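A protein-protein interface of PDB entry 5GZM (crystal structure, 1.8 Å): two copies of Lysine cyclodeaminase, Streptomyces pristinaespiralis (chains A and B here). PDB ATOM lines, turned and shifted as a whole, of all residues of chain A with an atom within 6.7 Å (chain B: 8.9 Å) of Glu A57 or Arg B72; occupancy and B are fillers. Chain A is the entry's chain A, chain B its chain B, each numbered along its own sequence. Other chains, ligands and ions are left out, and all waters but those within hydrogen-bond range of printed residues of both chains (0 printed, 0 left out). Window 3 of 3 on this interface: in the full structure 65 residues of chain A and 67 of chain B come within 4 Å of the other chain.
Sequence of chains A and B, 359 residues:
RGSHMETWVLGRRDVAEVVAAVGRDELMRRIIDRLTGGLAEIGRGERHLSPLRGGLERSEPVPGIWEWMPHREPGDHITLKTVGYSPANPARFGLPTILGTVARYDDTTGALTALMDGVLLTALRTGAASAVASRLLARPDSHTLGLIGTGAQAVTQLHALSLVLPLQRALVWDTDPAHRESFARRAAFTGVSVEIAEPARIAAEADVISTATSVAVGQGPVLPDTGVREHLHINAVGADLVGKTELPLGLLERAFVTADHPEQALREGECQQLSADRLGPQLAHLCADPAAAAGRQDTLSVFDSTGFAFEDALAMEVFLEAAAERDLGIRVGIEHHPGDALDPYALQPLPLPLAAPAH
The backbone carbonyl oxygen (O) of Glu A57 lies within hydrogen-bond range of the guanidinium group (NH1) of Arg B72 (3.4 Å).
The backbone carbonyl oxygen (O) of Thr B108 lies within hydrogen-bond range of the guanidinium group (NH1) of Arg A58 (3.0 Å).
NH1 of Arg A58 sits at hydrogen-bond distance from O of Asp B107 (2.7 Å).
The backbone NH of Asp B107 sits at hydrogen-bond distance from the backbone carbonyl oxygen of Asp B76 (3.1 Å).
NH2 of Arg A58 lies within hydrogen-bond range of O of Ile A65, 3.1 Å away.
N of Leu A56 is in hydrogen-bond range of O of Trp A66.
The backbone NH of Gly A64 sits at hydrogen-bond distance from the backbone carbonyl oxygen of Arg A58.
The side-chain carboxylate (OD2) of Asp B107 is in salt-bridge range of the guanidinium group (NH2) of Arg B72, 2.6 Å away.
O of Tyr B105 lies within hydrogen-bond range of N of Ile B78, 2.7 Å away.
Among the printed residues, pairs that only touch across the chains: Trp A66 with Tyr B105, Arg A58 with Arg B72, Trp A66 with Ile B78 and Leu A56 with Arg B72.
Of the printed residues of chain B, Trp A66 touches Ile B78 (3.7 Å) and Tyr B105 (3.4 Å).
Printed residues of chain A within 4 Å of Tyr B105: Trp A66.
Printed residues of chain B within 4 Å of Leu A56: Arg B72 (3.999 Å).
Of the printed residues of chain A, Thr B108 touches Arg A58.
Printed residues of chain B within 4 Å of Arg A58: Arg B72, Asp B107 and Thr B108.
Pro B74 touches none of the printed residues of chain A.
The nearest residue of chain B that does not touch Glu A57 is Asp B107 (6.0 Å).
The nearest printed residue of chain A that does not touch Arg B72 is Ser A59 (4.5 Å).
The nearest printed residue of chain B that does not touch Trp A66 is Leu B80 (4.1 Å).
Hydrophobic or aromatic side chains of chain B within 4 Å of the printed part of chain A: Ile B78 and Tyr B105.
Hydrophobic or aromatic side chains of chain A within 4 Å of the printed part of chain B: Leu A56 and Trp A66.
Among the printed residues, no Asp or Glu carboxylate lies within 4 Å of a Lys or Arg side-chain nitrogen of the other chain.
No position is printed for both chains.
Of the 7 pairs that touch across the chains among the printed residues, none has its exchanged pair printed and touching as well.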
ATOM      1  N   GLY A  55     -26.792   1.095  19.560  1.00  0.00           N
ATOM      2  CA  GLY A  55     -25.658   1.030  18.661  1.00  0.00           C
ATOM      3  C   GLY A  55     -25.996   0.954  17.198  1.00  0.00           C
ATOM      4  O   GLY A  55     -27.135   0.667  16.823  1.00  0.00           O
ATOM      5  N   LEU A  56     -24.994   1.222  16.392  1.00  0.00           N
ATOM      6  CA  LEU A  56     -25.115   1.236  14.945  1.00  0.00           C
ATOM      7  C   LEU A  56     -24.078   0.287  14.356  1.00  0.00           C
ATOM      8  O   LEU A  56     -22.878   0.493  14.503  1.00  0.00           O
ATOM      9  CB  LEU A  56     -24.836   2.633  14.440  1.00  0.00           C
ATOM     10  CG  LEU A  56     -25.882   3.653  14.858  1.00  0.00           C
ATOM     11  CD1 LEU A  56     -25.427   5.043  14.440  1.00  0.00           C
ATOM     12  CD2 LEU A  56     -27.259   3.307  14.302  1.00  0.00           C
ATOM     13  N   GLU A  57     -24.573  -0.762  13.713  1.00  0.00           N
ATOM     14  CA  GLU A  57     -23.700  -1.695  13.030  1.00  0.00           C
ATOM     15  C   GLU A  57     -23.051  -0.984  11.862  1.00  0.00           C
ATOM     16  O   GLU A  57     -23.709  -0.251  11.128  1.00  0.00           O
ATOM     17  CB  GLU A  57     -24.476  -2.917  12.566  1.00  0.00           C
ATOM     18  CG  GLU A  57     -24.947  -3.805  13.710  1.00  0.00           C
ATOM     19  CD  GLU A  57     -25.183  -5.233  13.252  1.00  0.00           C
ATOM     20  OE1 GLU A  57     -26.061  -5.449  12.394  1.00  0.00           O
ATOM     21  OE2 GLU A  57     -24.482  -6.143  13.737  1.00  0.00           O
ATOM     22  N   ARG A  58     -21.742  -1.162  11.740  1.00  0.00           N
ATOM     23  CA  ARG A  58     -20.985  -0.767  10.585  1.00  0.00           C
ATOM     24  C   ARG A  58     -20.445  -2.008   9.829  1.00  0.00           C
ATOM     25  O   ARG A  58     -19.928  -2.950  10.419  1.00  0.00           O
ATOM     26  CB  ARG A  58     -19.867   0.189  10.983  1.00  0.00           C
ATOM     27  CG  ARG A  58     -20.396   1.565  11.464  1.00  0.00           C
ATOM     28  CD  ARG A  58     -19.294   2.491  12.006  1.00  0.00           C
ATOM     29  NE  ARG A  58     -18.752   1.802  13.106  1.00  0.00           N
ATOM     30  CZ  ARG A  58     -17.481   1.695  13.522  1.00  0.00           C
ATOM     31  NH1 ARG A  58     -16.453   2.396  13.100  1.00  0.00           N
ATOM     32  NH2 ARG A  58     -17.291   0.869  14.508  1.00  0.00           N
ATOM     33  N   SER A  59     -20.582  -1.992   8.514  1.00  0.00           N
ATOM     34  CA  SER A  59     -20.246  -3.147   7.681  1.00  0.00           C
ATOM     35  C   SER A  59     -18.797  -3.127   7.240  1.00  0.00           C
ATOM     36  O   SER A  59     -18.187  -4.185   7.024  1.00  0.00           O
ATOM     37  CB  SER A  59     -21.120  -3.152   6.426  1.00  0.00           C
ATOM     38  OG  SER A  59     -22.348  -3.773   6.698  1.00  0.00           O
ATOM     39  N   GLU A  60     -18.250  -1.933   7.096  1.00  0.00           N
ATOM     40  CA  GLU A  60     -16.973  -1.733   6.415  1.00  0.00           C
ATOM     41  C   GLU A  60     -16.061  -0.984   7.322  1.00  0.00           C
ATOM     42  O   GLU A  60     -16.540  -0.184   8.079  1.00  0.00           O
ATOM     43  CB  GLU A  60     -17.151  -0.855   5.175  1.00  0.00           C
ATOM     44  CG  GLU A  60     -18.204  -1.359   4.210  1.00  0.00           C
ATOM     45  CD  GLU A  60     -17.621  -2.197   3.125  1.00  0.00           C
ATOM     46  OE1 GLU A  60     -16.414  -2.032   2.854  1.00  0.00           O
ATOM     47  OE2 GLU A  60     -18.370  -3.004   2.545  1.00  0.00           O
ATOM     48  N   PRO A  63     -16.911  -5.923   9.775  1.00  0.00           N
ATOM     49  CA  PRO A  63     -18.030  -5.655  10.629  1.00  0.00           C
ATOM     50  C   PRO A  63     -17.628  -5.110  12.007  1.00  0.00           C
ATOM     51  O   PRO A  63     -16.716  -5.633  12.682  1.00  0.00           O
ATOM     52  CB  PRO A  63     -18.755  -7.009  10.667  1.00  0.00           C
ATOM     53  CG  PRO A  63     -18.555  -7.540   9.265  1.00  0.00           C
ATOM     54  CD  PRO A  63     -17.129  -7.149   8.975  1.00  0.00           C
ATOM     55  N   GLY A  64     -18.274  -4.006  12.377  1.00  0.00           N
ATOM     56  CA  GLY A  64     -18.038  -3.333  13.664  1.00  0.00           C
ATOM     57  C   GLY A  64     -19.320  -2.721  14.192  1.00  0.00           C
ATOM     58  O   GLY A  64     -20.420  -2.912  13.612  1.00  0.00           O
ATOM     59  N   ILE A  65     -19.191  -2.011  15.314  1.00  0.00           N
ATOM     60  CA  ILE A  65     -20.348  -1.424  15.985  1.00  0.00           C
ATOM     61  C   ILE A  65     -19.908  -0.094  16.671  1.00  0.00           C
ATOM     62  O   ILE A  65     -18.786   0.046  17.138  1.00  0.00           O
ATOM     63  CB  ILE A  65     -21.079  -2.435  16.902  1.00  0.00           C
ATOM     64  CG1 ILE A  65     -22.458  -1.910  17.323  1.00  0.00           C
ATOM     65  CG2 ILE A  65     -20.289  -2.844  18.141  1.00  0.00           C
ATOM     66  CD1 ILE A  65     -23.529  -2.977  17.561  1.00  0.00           C
ATOM     67  N   TRP A  66     -20.811   0.871  16.728  1.00  0.00           N
ATOM     68  CA  TRP A  66     -20.569   2.141  17.433  1.00  0.00           C
ATOM     69  C   TRP A  66     -21.766   2.270  18.369  1.00  0.00           C
ATOM     70  O   TRP A  66     -22.895   2.232  17.920  1.00  0.00           O
ATOM     71  CB  TRP A  66     -20.505   3.356  16.511  1.00  0.00           C
ATOM     72  CG  TRP A  66     -20.167   4.599  17.217  1.00  0.00           C
ATOM     73  CD1 TRP A  66     -18.930   5.000  17.612  1.00  0.00           C
ATOM     74  CD2 TRP A  66     -21.092   5.608  17.734  1.00  0.00           C
ATOM     75  NE1 TRP A  66     -19.009   6.167  18.312  1.00  0.00           N
ATOM     76  CE2 TRP A  66     -20.305   6.590  18.370  1.00  0.00           C
ATOM     77  CE3 TRP A  66     -22.452   5.804  17.633  1.00  0.00           C
ATOM     78  CZ2 TRP A  66     -20.850   7.752  18.939  1.00  0.00           C
ATOM     79  CZ3 TRP A  66     -22.995   6.983  18.189  1.00  0.00           C
ATOM     80  CH2 TRP A  66     -22.182   7.908  18.851  1.00  0.00           C
ATOM     81  N   VAL A 217     -17.731 -12.439  13.784  1.00  0.00           N
ATOM     82  CA  VAL A 217     -18.986 -13.191  13.928  1.00  0.00           C
ATOM     83  C   VAL A 217     -18.909 -14.574  13.260  1.00  0.00           C
ATOM     84  O   VAL A 217     -18.462 -14.688  12.145  1.00  0.00           O
ATOM     85  CB  VAL A 217     -20.166 -12.372  13.347  1.00  0.00           C
ATOM     86  CG1 VAL A 217     -21.403 -13.224  13.106  1.00  0.00           C
ATOM     87  CG2 VAL A 217     -20.487 -11.190  14.260  1.00  0.00           C
ATOM     88  N   LEU A 241     -20.533  -7.718  18.342  1.00  0.00           N
ATOM     89  CA  LEU A 241     -21.674  -8.065  17.534  1.00  0.00           C
ATOM     90  C   LEU A 241     -22.463  -9.289  18.047  1.00  0.00           C
ATOM     91  O   LEU A 241     -21.963 -10.159  18.779  1.00  0.00           O
ATOM     92  CB  LEU A 241     -21.190  -8.282  16.116  1.00  0.00           C
ATOM     93  CG  LEU A 241     -20.579  -7.028  15.528  1.00  0.00           C
ATOM     94  CD1 LEU A 241     -19.745  -7.345  14.279  1.00  0.00           C
ATOM     95  CD2 LEU A 241     -21.723  -6.078  15.222  1.00  0.00           C
ATOM     96  N   VAL A 242     -23.738  -9.296  17.720  1.00  0.00           N
ATOM     97  CA  VAL A 242     -24.580 -10.439  17.993  1.00  0.00           C
ATOM     98  C   VAL A 242     -23.960 -11.412  17.025  1.00  0.00           C
ATOM     99  O   VAL A 242     -23.563 -11.018  15.902  1.00  0.00           O
ATOM    100  CB  VAL A 242     -26.046 -10.132  17.606  1.00  0.00           C
ATOM    101  CG1 VAL A 242     -26.862 -11.411  17.411  1.00  0.00           C
ATOM    102  CG2 VAL A 242     -26.666  -9.252  18.667  1.00  0.00           C
ATOM    103  N   ARG B  47     -31.234   9.524   0.953  1.00  0.00           N
ATOM    104  CA  ARG B  47     -30.766   9.540   2.335  1.00  0.00           C
ATOM    105  C   ARG B  47     -31.956   9.069   3.165  1.00  0.00           C
ATOM    106  O   ARG B  47     -33.100   9.049   2.675  1.00  0.00           O
ATOM    107  CB  ARG B  47     -30.319  10.959   2.755  1.00  0.00           C
ATOM    108  CG  ARG B  47     -29.176  11.538   1.921  1.00  0.00           C
ATOM    109  CD  ARG B  47     -28.086  12.202   2.757  1.00  0.00           C
ATOM    110  NE  ARG B  47     -27.993  13.646   2.546  1.00  0.00           N
ATOM    111  CZ  ARG B  47     -27.156  14.467   3.189  1.00  0.00           C
ATOM    112  NH1 ARG B  47     -26.328  14.013   4.122  1.00  0.00           N
ATOM    113  NH2 ARG B  47     -27.151  15.759   2.897  1.00  0.00           N
ATOM    114  N   HIS B  48     -31.708   8.684   4.419  1.00  0.00           N
ATOM    115  CA  HIS B  48     -32.771   8.135   5.280  1.00  0.00           C
ATOM    116  C   HIS B  48     -33.053   9.025   6.501  1.00  0.00           C
ATOM    117  O   HIS B  48     -32.184   9.786   6.928  1.00  0.00           O
ATOM    118  CB  HIS B  48     -32.379   6.734   5.786  1.00  0.00           C
ATOM    119  CG  HIS B  48     -32.325   5.694   4.708  1.00  0.00           C
ATOM    120  ND1 HIS B  48     -31.623   5.872   3.534  1.00  0.00           N
ATOM    121  CD2 HIS B  48     -32.881   4.461   4.633  1.00  0.00           C
ATOM    122  CE1 HIS B  48     -31.754   4.799   2.775  1.00  0.00           C
ATOM    123  NE2 HIS B  48     -32.505   3.925   3.423  1.00  0.00           N
ATOM    124  N   LEU B  49     -34.275   8.936   7.003  1.00  0.00           N
ATOM    125  CA  LEU B  49     -34.670   9.609   8.230  1.00  0.00           C
ATOM    126  C   LEU B  49     -33.808   9.005   9.309  1.00  0.00           C
ATOM    127  O   LEU B  49     -33.531   7.818   9.273  1.00  0.00           O
ATOM    128  CB  LEU B  49     -36.126   9.335   8.560  1.00  0.00           C
ATOM    129  CG  LEU B  49     -37.187  10.077   7.756  1.00  0.00           C
ATOM    130  CD1 LEU B  49     -38.533   9.448   7.997  1.00  0.00           C
ATOM    131  CD2 LEU B  49     -37.214  11.563   8.091  1.00  0.00           C
ATOM    132  N   SER B  50     -33.361   9.825  10.231  1.00  0.00           N
ATOM    133  CA  SER B  50     -32.718   9.314  11.429  1.00  0.00           C
ATOM    134  C   SER B  50     -33.519   8.201  12.164  1.00  0.00           C
ATOM    135  O   SER B  50     -34.745   8.185  12.184  1.00  0.00           O
ATOM    136  CB  SER B  50     -32.555  10.497  12.335  1.00  0.00           C
ATOM    137  OG  SER B  50     -31.828  11.507  11.717  1.00  0.00           O
ATOM    138  N   PRO B  51     -32.806   7.302  12.893  1.00  0.00           N
ATOM    139  CA  PRO B  51     -33.528   6.319  13.644  1.00  0.00           C
ATOM    140  C   PRO B  51     -34.265   6.969  14.839  1.00  0.00           C
ATOM    141  O   PRO B  51     -34.024   8.134  15.195  1.00  0.00           O
ATOM    142  CB  PRO B  51     -32.433   5.335  14.082  1.00  0.00           C
ATOM    143  CG  PRO B  51     -31.196   6.142  14.153  1.00  0.00           C
ATOM    144  CD  PRO B  51     -31.352   7.237  13.113  1.00  0.00           C
ATOM    145  N   MET B  69     -29.662  11.574  20.211  1.00  0.00           N
ATOM    146  CA  MET B  69     -30.194  11.616  18.856  1.00  0.00           C
ATOM    147  C   MET B  69     -29.069  11.351  17.866  1.00  0.00           C
ATOM    148  O   MET B  69     -28.315  12.266  17.512  1.00  0.00           O
ATOM    149  CB  MET B  69     -30.827  12.972  18.569  1.00  0.00           C
ATOM    150  CG  MET B  69     -32.007  13.263  19.494  1.00  0.00           C
ATOM    151  SD  MET B  69     -32.576  14.998  19.459  1.00  0.00           S
ATOM    152  CE  MET B  69     -33.130  15.084  17.739  1.00  0.00           C
ATOM    153  N   PRO B  70     -28.936  10.096  17.433  1.00  0.00           N
ATOM    154  CA  PRO B  70     -27.933   9.712  16.432  1.00  0.00           C
ATOM    155  C   PRO B  70     -28.402   9.807  14.985  1.00  0.00           C
ATOM    156  O   PRO B  70     -29.589   9.533  14.708  1.00  0.00           O
ATOM    157  CB  PRO B  70     -27.635   8.238  16.772  1.00  0.00           C
ATOM    158  CG  PRO B  70     -28.837   7.775  17.486  1.00  0.00           C
ATOM    159  CD  PRO B  70     -29.590   8.949  18.053  1.00  0.00           C
ATOM    160  N   HIS B  71     -27.472  10.206  14.125  1.00  0.00           N
ATOM    161  CA  HIS B  71     -27.599  10.119  12.653  1.00  0.00           C
ATOM    162  C   HIS B  71     -26.278   9.670  12.001  1.00  0.00           C
ATOM    163  O   HIS B  71     -25.267  10.340  12.120  1.00  0.00           O
ATOM    164  CB  HIS B  71     -27.947  11.451  12.017  1.00  0.00           C
ATOM    165  CG  HIS B  71     -28.386  11.306  10.605  1.00  0.00           C
ATOM    166  ND1 HIS B  71     -29.609  10.769  10.271  1.00  0.00           N
ATOM    167  CD2 HIS B  71     -27.718  11.493   9.440  1.00  0.00           C
ATOM    168  CE1 HIS B  71     -29.678  10.630   8.956  1.00  0.00           C
ATOM    169  NE2 HIS B  71     -28.554  11.081   8.430  1.00  0.00           N
ATOM    170  N   ARG B  72     -26.354   8.558  11.269  1.00  0.00           N
ATOM    171  CA  ARG B  72     -25.190   8.016  10.576  1.00  0.00           C
ATOM    172  C   ARG B  72     -25.215   8.347   9.088  1.00  0.00           C
ATOM    173  O   ARG B  72     -26.202   8.095   8.430  1.00  0.00           O
ATOM    174  CB  ARG B  72     -25.166   6.509  10.729  1.00  0.00           C
ATOM    175  CG  ARG B  72     -23.883   5.880  10.197  1.00  0.00           C
ATOM    176  CD  ARG B  72     -23.787   4.440  10.640  1.00  0.00           C
ATOM    177  NE  ARG B  72     -22.707   3.825   9.876  1.00  0.00           N
ATOM    178  CZ  ARG B  72     -22.823   2.814   9.011  1.00  0.00           C
ATOM    179  NH1 ARG B  72     -23.971   2.191   8.790  1.00  0.00           N
ATOM    180  NH2 ARG B  72     -21.740   2.394   8.384  1.00  0.00           N
ATOM    181  N   GLU B  73     -24.123   8.863   8.576  1.00  0.00           N
ATOM    182  CA  GLU B  73     -23.917   8.821   7.132  1.00  0.00           C
ATOM    183  C   GLU B  73     -22.923   7.675   6.819  1.00  0.00           C
ATOM    184  O   GLU B  73     -21.755   7.844   7.032  1.00  0.00           O
ATOM    185  CB  GLU B  73     -23.447  10.183   6.656  1.00  0.00           C
ATOM    186  CG  GLU B  73     -24.592  11.228   6.607  1.00  0.00           C
ATOM    187  CD  GLU B  73     -25.707  10.891   5.592  1.00  0.00           C
ATOM    188  OE1 GLU B  73     -26.938  11.058   5.914  1.00  0.00           O
ATOM    189  OE2 GLU B  73     -25.355  10.473   4.455  1.00  0.00           O
ATOM    190  N   PRO B  74     -23.411   6.500   6.394  1.00  0.00           N
ATOM    191  CA  PRO B  74     -22.426   5.411   6.346  1.00  0.00           C
ATOM    192  C   PRO B  74     -21.206   5.803   5.560  1.00  0.00           C
ATOM    193  O   PRO B  74     -21.335   6.185   4.413  1.00  0.00           O
ATOM    194  CB  PRO B  74     -23.183   4.268   5.673  1.00  0.00           C
ATOM    195  CG  PRO B  74     -24.631   4.567   5.871  1.00  0.00           C
ATOM    196  CD  PRO B  74     -24.749   6.052   5.966  1.00  0.00           C
ATOM    197  N   GLY B  75     -20.037   5.789   6.201  1.00  0.00           N
ATOM    198  CA  GLY B  75     -18.767   6.023   5.531  1.00  0.00           C
ATOM    199  C   GLY B  75     -18.097   7.359   5.747  1.00  0.00           C
ATOM    200  O   GLY B  75     -16.937   7.465   5.490  1.00  0.00           O
ATOM    201  N   ASP B  76     -18.809   8.395   6.205  1.00  0.00           N
ATOM    202  CA  ASP B  76     -18.169   9.675   6.547  1.00  0.00           C
ATOM    203  C   ASP B  76     -18.182   9.785   8.084  1.00  0.00           C
ATOM    204  O   ASP B  76     -17.142   9.716   8.707  1.00  0.00           O
ATOM    205  CB  ASP B  76     -18.901  10.891   5.866  1.00  0.00           C
ATOM    206  CG  ASP B  76     -18.142  12.261   5.998  1.00  0.00           C
ATOM    207  OD1 ASP B  76     -17.183  12.438   6.776  1.00  0.00           O
ATOM    208  OD2 ASP B  76     -18.537  13.227   5.308  1.00  0.00           O
ATOM    209  N   HIS B  77     -19.367   9.993   8.670  1.00  0.00           N
ATOM    210  CA  HIS B  77     -19.419  10.305  10.089  1.00  0.00           C
ATOM    211  C   HIS B  77     -20.757   9.983  10.716  1.00  0.00           C
ATOM    212  O   HIS B  77     -21.762   9.664  10.061  1.00  0.00           O
ATOM    213  CB  HIS B  77     -18.910  11.746  10.395  1.00  0.00           C
ATOM    214  CG  HIS B  77     -19.791  12.823   9.849  1.00  0.00           C
ATOM    215  ND1 HIS B  77     -19.485  13.518   8.694  1.00  0.00           N
ATOM    216  CD2 HIS B  77     -20.967  13.321  10.290  1.00  0.00           C
ATOM    217  CE1 HIS B  77     -20.439  14.400   8.452  1.00  0.00           C
ATOM    218  NE2 HIS B  77     -21.349  14.303   9.407  1.00  0.00           N
ATOM    219  N   ILE B  78     -20.724   9.949  12.048  1.00  0.00           N
ATOM    220  CA  ILE B  78     -21.907   9.730  12.859  1.00  0.00           C
ATOM    221  C   ILE B  78     -22.059  11.021  13.678  1.00  0.00           C
ATOM    222  O   ILE B  78     -21.091  11.543  14.268  1.00  0.00           O
ATOM    223  CB  ILE B  78     -21.765   8.521  13.819  1.00  0.00           C
ATOM    224  CG1 ILE B  78     -21.656   7.199  13.032  1.00  0.00           C
ATOM    225  CG2 ILE B  78     -22.965   8.479  14.773  1.00  0.00           C
ATOM    226  CD1 ILE B  78     -21.331   5.958  13.863  1.00  0.00           C
ATOM    227  N   THR B  79     -23.266  11.558  13.691  1.00  0.00           N
ATOM    228  CA  THR B  79     -23.571  12.731  14.500  1.00  0.00           C
ATOM    229  C   THR B  79     -24.401  12.220  15.669  1.00  0.00           C
ATOM    230  O   THR B  79     -25.278  11.366  15.507  1.00  0.00           O
ATOM    231  CB  THR B  79     -24.413  13.764  13.732  1.00  0.00           C
ATOM    232  OG1 THR B  79     -23.719  14.190  12.532  1.00  0.00           O
ATOM    233  CG2 THR B  79     -24.645  15.010  14.616  1.00  0.00           C
ATOM    234  N   LEU B  80     -24.052  12.683  16.863  1.00  0.00           N
ATOM    235  CA  LEU B  80     -24.862  12.443  18.056  1.00  0.00           C
ATOM    236  C   LEU B  80     -25.171  13.787  18.766  1.00  0.00           C
ATOM    237  O   LEU B  80     -24.223  14.487  19.183  1.00  0.00           O
ATOM    238  CB  LEU B  80     -24.115  11.532  19.048  1.00  0.00           C
ATOM    239  CG  LEU B  80     -24.986  11.185  20.242  1.00  0.00           C
ATOM    240  CD1 LEU B  80     -26.052  10.198  19.821  1.00  0.00           C
ATOM    241  CD2 LEU B  80     -24.105  10.577  21.325  1.00  0.00           C
ATOM    242  N   TYR B 105     -18.432  11.944  15.034  1.00  0.00           N
ATOM    243  CA  TYR B 105     -17.463  10.814  15.108  1.00  0.00           C
ATOM    244  C   TYR B 105     -17.224  10.229  13.699  1.00  0.00           C
ATOM    245  O   TYR B 105     -18.153  10.029  12.960  1.00  0.00           O
ATOM    246  CB  TYR B 105     -18.050   9.688  15.948  1.00  0.00           C
ATOM    247  CG  TYR B 105     -18.455  10.126  17.333  1.00  0.00           C
ATOM    248  CD1 TYR B 105     -19.732  10.658  17.556  1.00  0.00           C
ATOM    249  CD2 TYR B 105     -17.594   9.970  18.421  1.00  0.00           C
ATOM    250  CE1 TYR B 105     -20.101  11.095  18.816  1.00  0.00           C
ATOM    251  CE2 TYR B 105     -17.983  10.360  19.710  1.00  0.00           C
ATOM    252  CZ  TYR B 105     -19.241  10.933  19.887  1.00  0.00           C
ATOM    253  OH  TYR B 105     -19.672  11.385  21.114  1.00  0.00           O
ATOM    254  N   ASP B 106     -15.983   9.879  13.383  1.00  0.00           N
ATOM    255  CA  ASP B 106     -15.686   9.169  12.101  1.00  0.00           C
ATOM    256  C   ASP B 106     -16.346   7.801  11.995  1.00  0.00           C
ATOM    257  O   ASP B 106     -16.214   7.012  12.933  1.00  0.00           O
ATOM    258  CB  ASP B 106     -14.178   9.086  11.959  1.00  0.00           C
ATOM    259  CG  ASP B 106     -13.778   8.527  10.619  1.00  0.00           C
ATOM    260  OD1 ASP B 106     -13.948   7.292  10.433  1.00  0.00           O
ATOM    261  OD2 ASP B 106     -13.419   9.347   9.726  1.00  0.00           O
ATOM    262  N   ASP B 107     -17.083   7.493  10.916  1.00  0.00           N
ATOM    263  CA  ASP B 107     -17.856   6.263  10.851  1.00  0.00           C
ATOM    264  C   ASP B 107     -16.845   5.142  10.747  1.00  0.00           C
ATOM    265  O   ASP B 107     -17.168   4.023  11.063  1.00  0.00           O
ATOM    266  CB  ASP B 107     -18.776   6.138   9.620  1.00  0.00           C
ATOM    267  CG  ASP B 107     -19.754   4.975   9.710  1.00  0.00           C
ATOM    268  OD1 ASP B 107     -20.474   4.831  10.748  1.00  0.00           O
ATOM    269  OD2 ASP B 107     -19.887   4.170   8.727  1.00  0.00           O
ATOM    270  N   THR B 108     -15.674   5.423  10.210  1.00  0.00           N
ATOM    271  CA  THR B 108     -14.855   4.279   9.786  1.00  0.00           C
ATOM    272  C   THR B 108     -14.080   3.719  10.974  1.00  0.00           C
ATOM    273  O   THR B 108     -14.110   2.506  11.210  1.00  0.00           O
ATOM    274  CB  THR B 108     -14.004   4.557   8.507  1.00  0.00           C
ATOM    275  OG1 THR B 108     -13.240   5.781   8.610  1.00  0.00           O
ATOM    276  CG2 THR B 108     -14.896   4.622   7.333  1.00  0.00           C
ATOM    277  N   ALA B 309     -32.197  14.063  14.313  1.00  0.00           N
ATOM    278  CA  ALA B 309     -30.773  14.287  14.285  1.00  0.00           C
ATOM    279  C   ALA B 309     -30.167  14.711  12.933  1.00  0.00           C
ATOM    280  O   ALA B 309     -29.180  15.446  12.892  1.00  0.00           O
ATOM    281  CB  ALA B 309     -30.069  13.047  14.815  1.00  0.00           C
ATOM    282  N   PHE B 310     -30.802  14.311  11.835  1.00  0.00           N
ATOM    283  CA  PHE B 310     -30.348  14.703  10.494  1.00  0.00           C
ATOM    284  C   PHE B 310     -30.326  16.210  10.430  1.00  0.00           C
ATOM    285  O   PHE B 310     -29.434  16.804   9.884  1.00  0.00           O
ATOM    286  CB  PHE B 310     -31.294  14.100   9.458  1.00  0.00           C
ATOM    287  CG  PHE B 310     -30.966  14.449   8.014  1.00  0.00           C
ATOM    288  CD1 PHE B 310     -29.796  14.024   7.436  1.00  0.00           C
ATOM    289  CD2 PHE B 310     -31.822  15.219   7.260  1.00  0.00           C
ATOM    290  CE1 PHE B 310     -29.486  14.323   6.112  1.00  0.00           C
ATOM    291  CE2 PHE B 310     -31.528  15.508   5.930  1.00  0.00           C
ATOM    292  CZ  PHE B 310     -30.369  15.040   5.358  1.00  0.00           C
ATOM    293  N   ALA B 313     -27.199  17.412  12.224  1.00  0.00           N
ATOM    294  CA  ALA B 313     -25.974  17.130  11.439  1.00  0.00           C
ATOM    295  C   ALA B 313     -25.741  18.203  10.410  1.00  0.00           C
ATOM    296  O   ALA B 313     -24.662  18.691  10.245  1.00  0.00           O
ATOM    297  CB  ALA B 313     -26.118  15.794  10.728  1.00  0.00           C
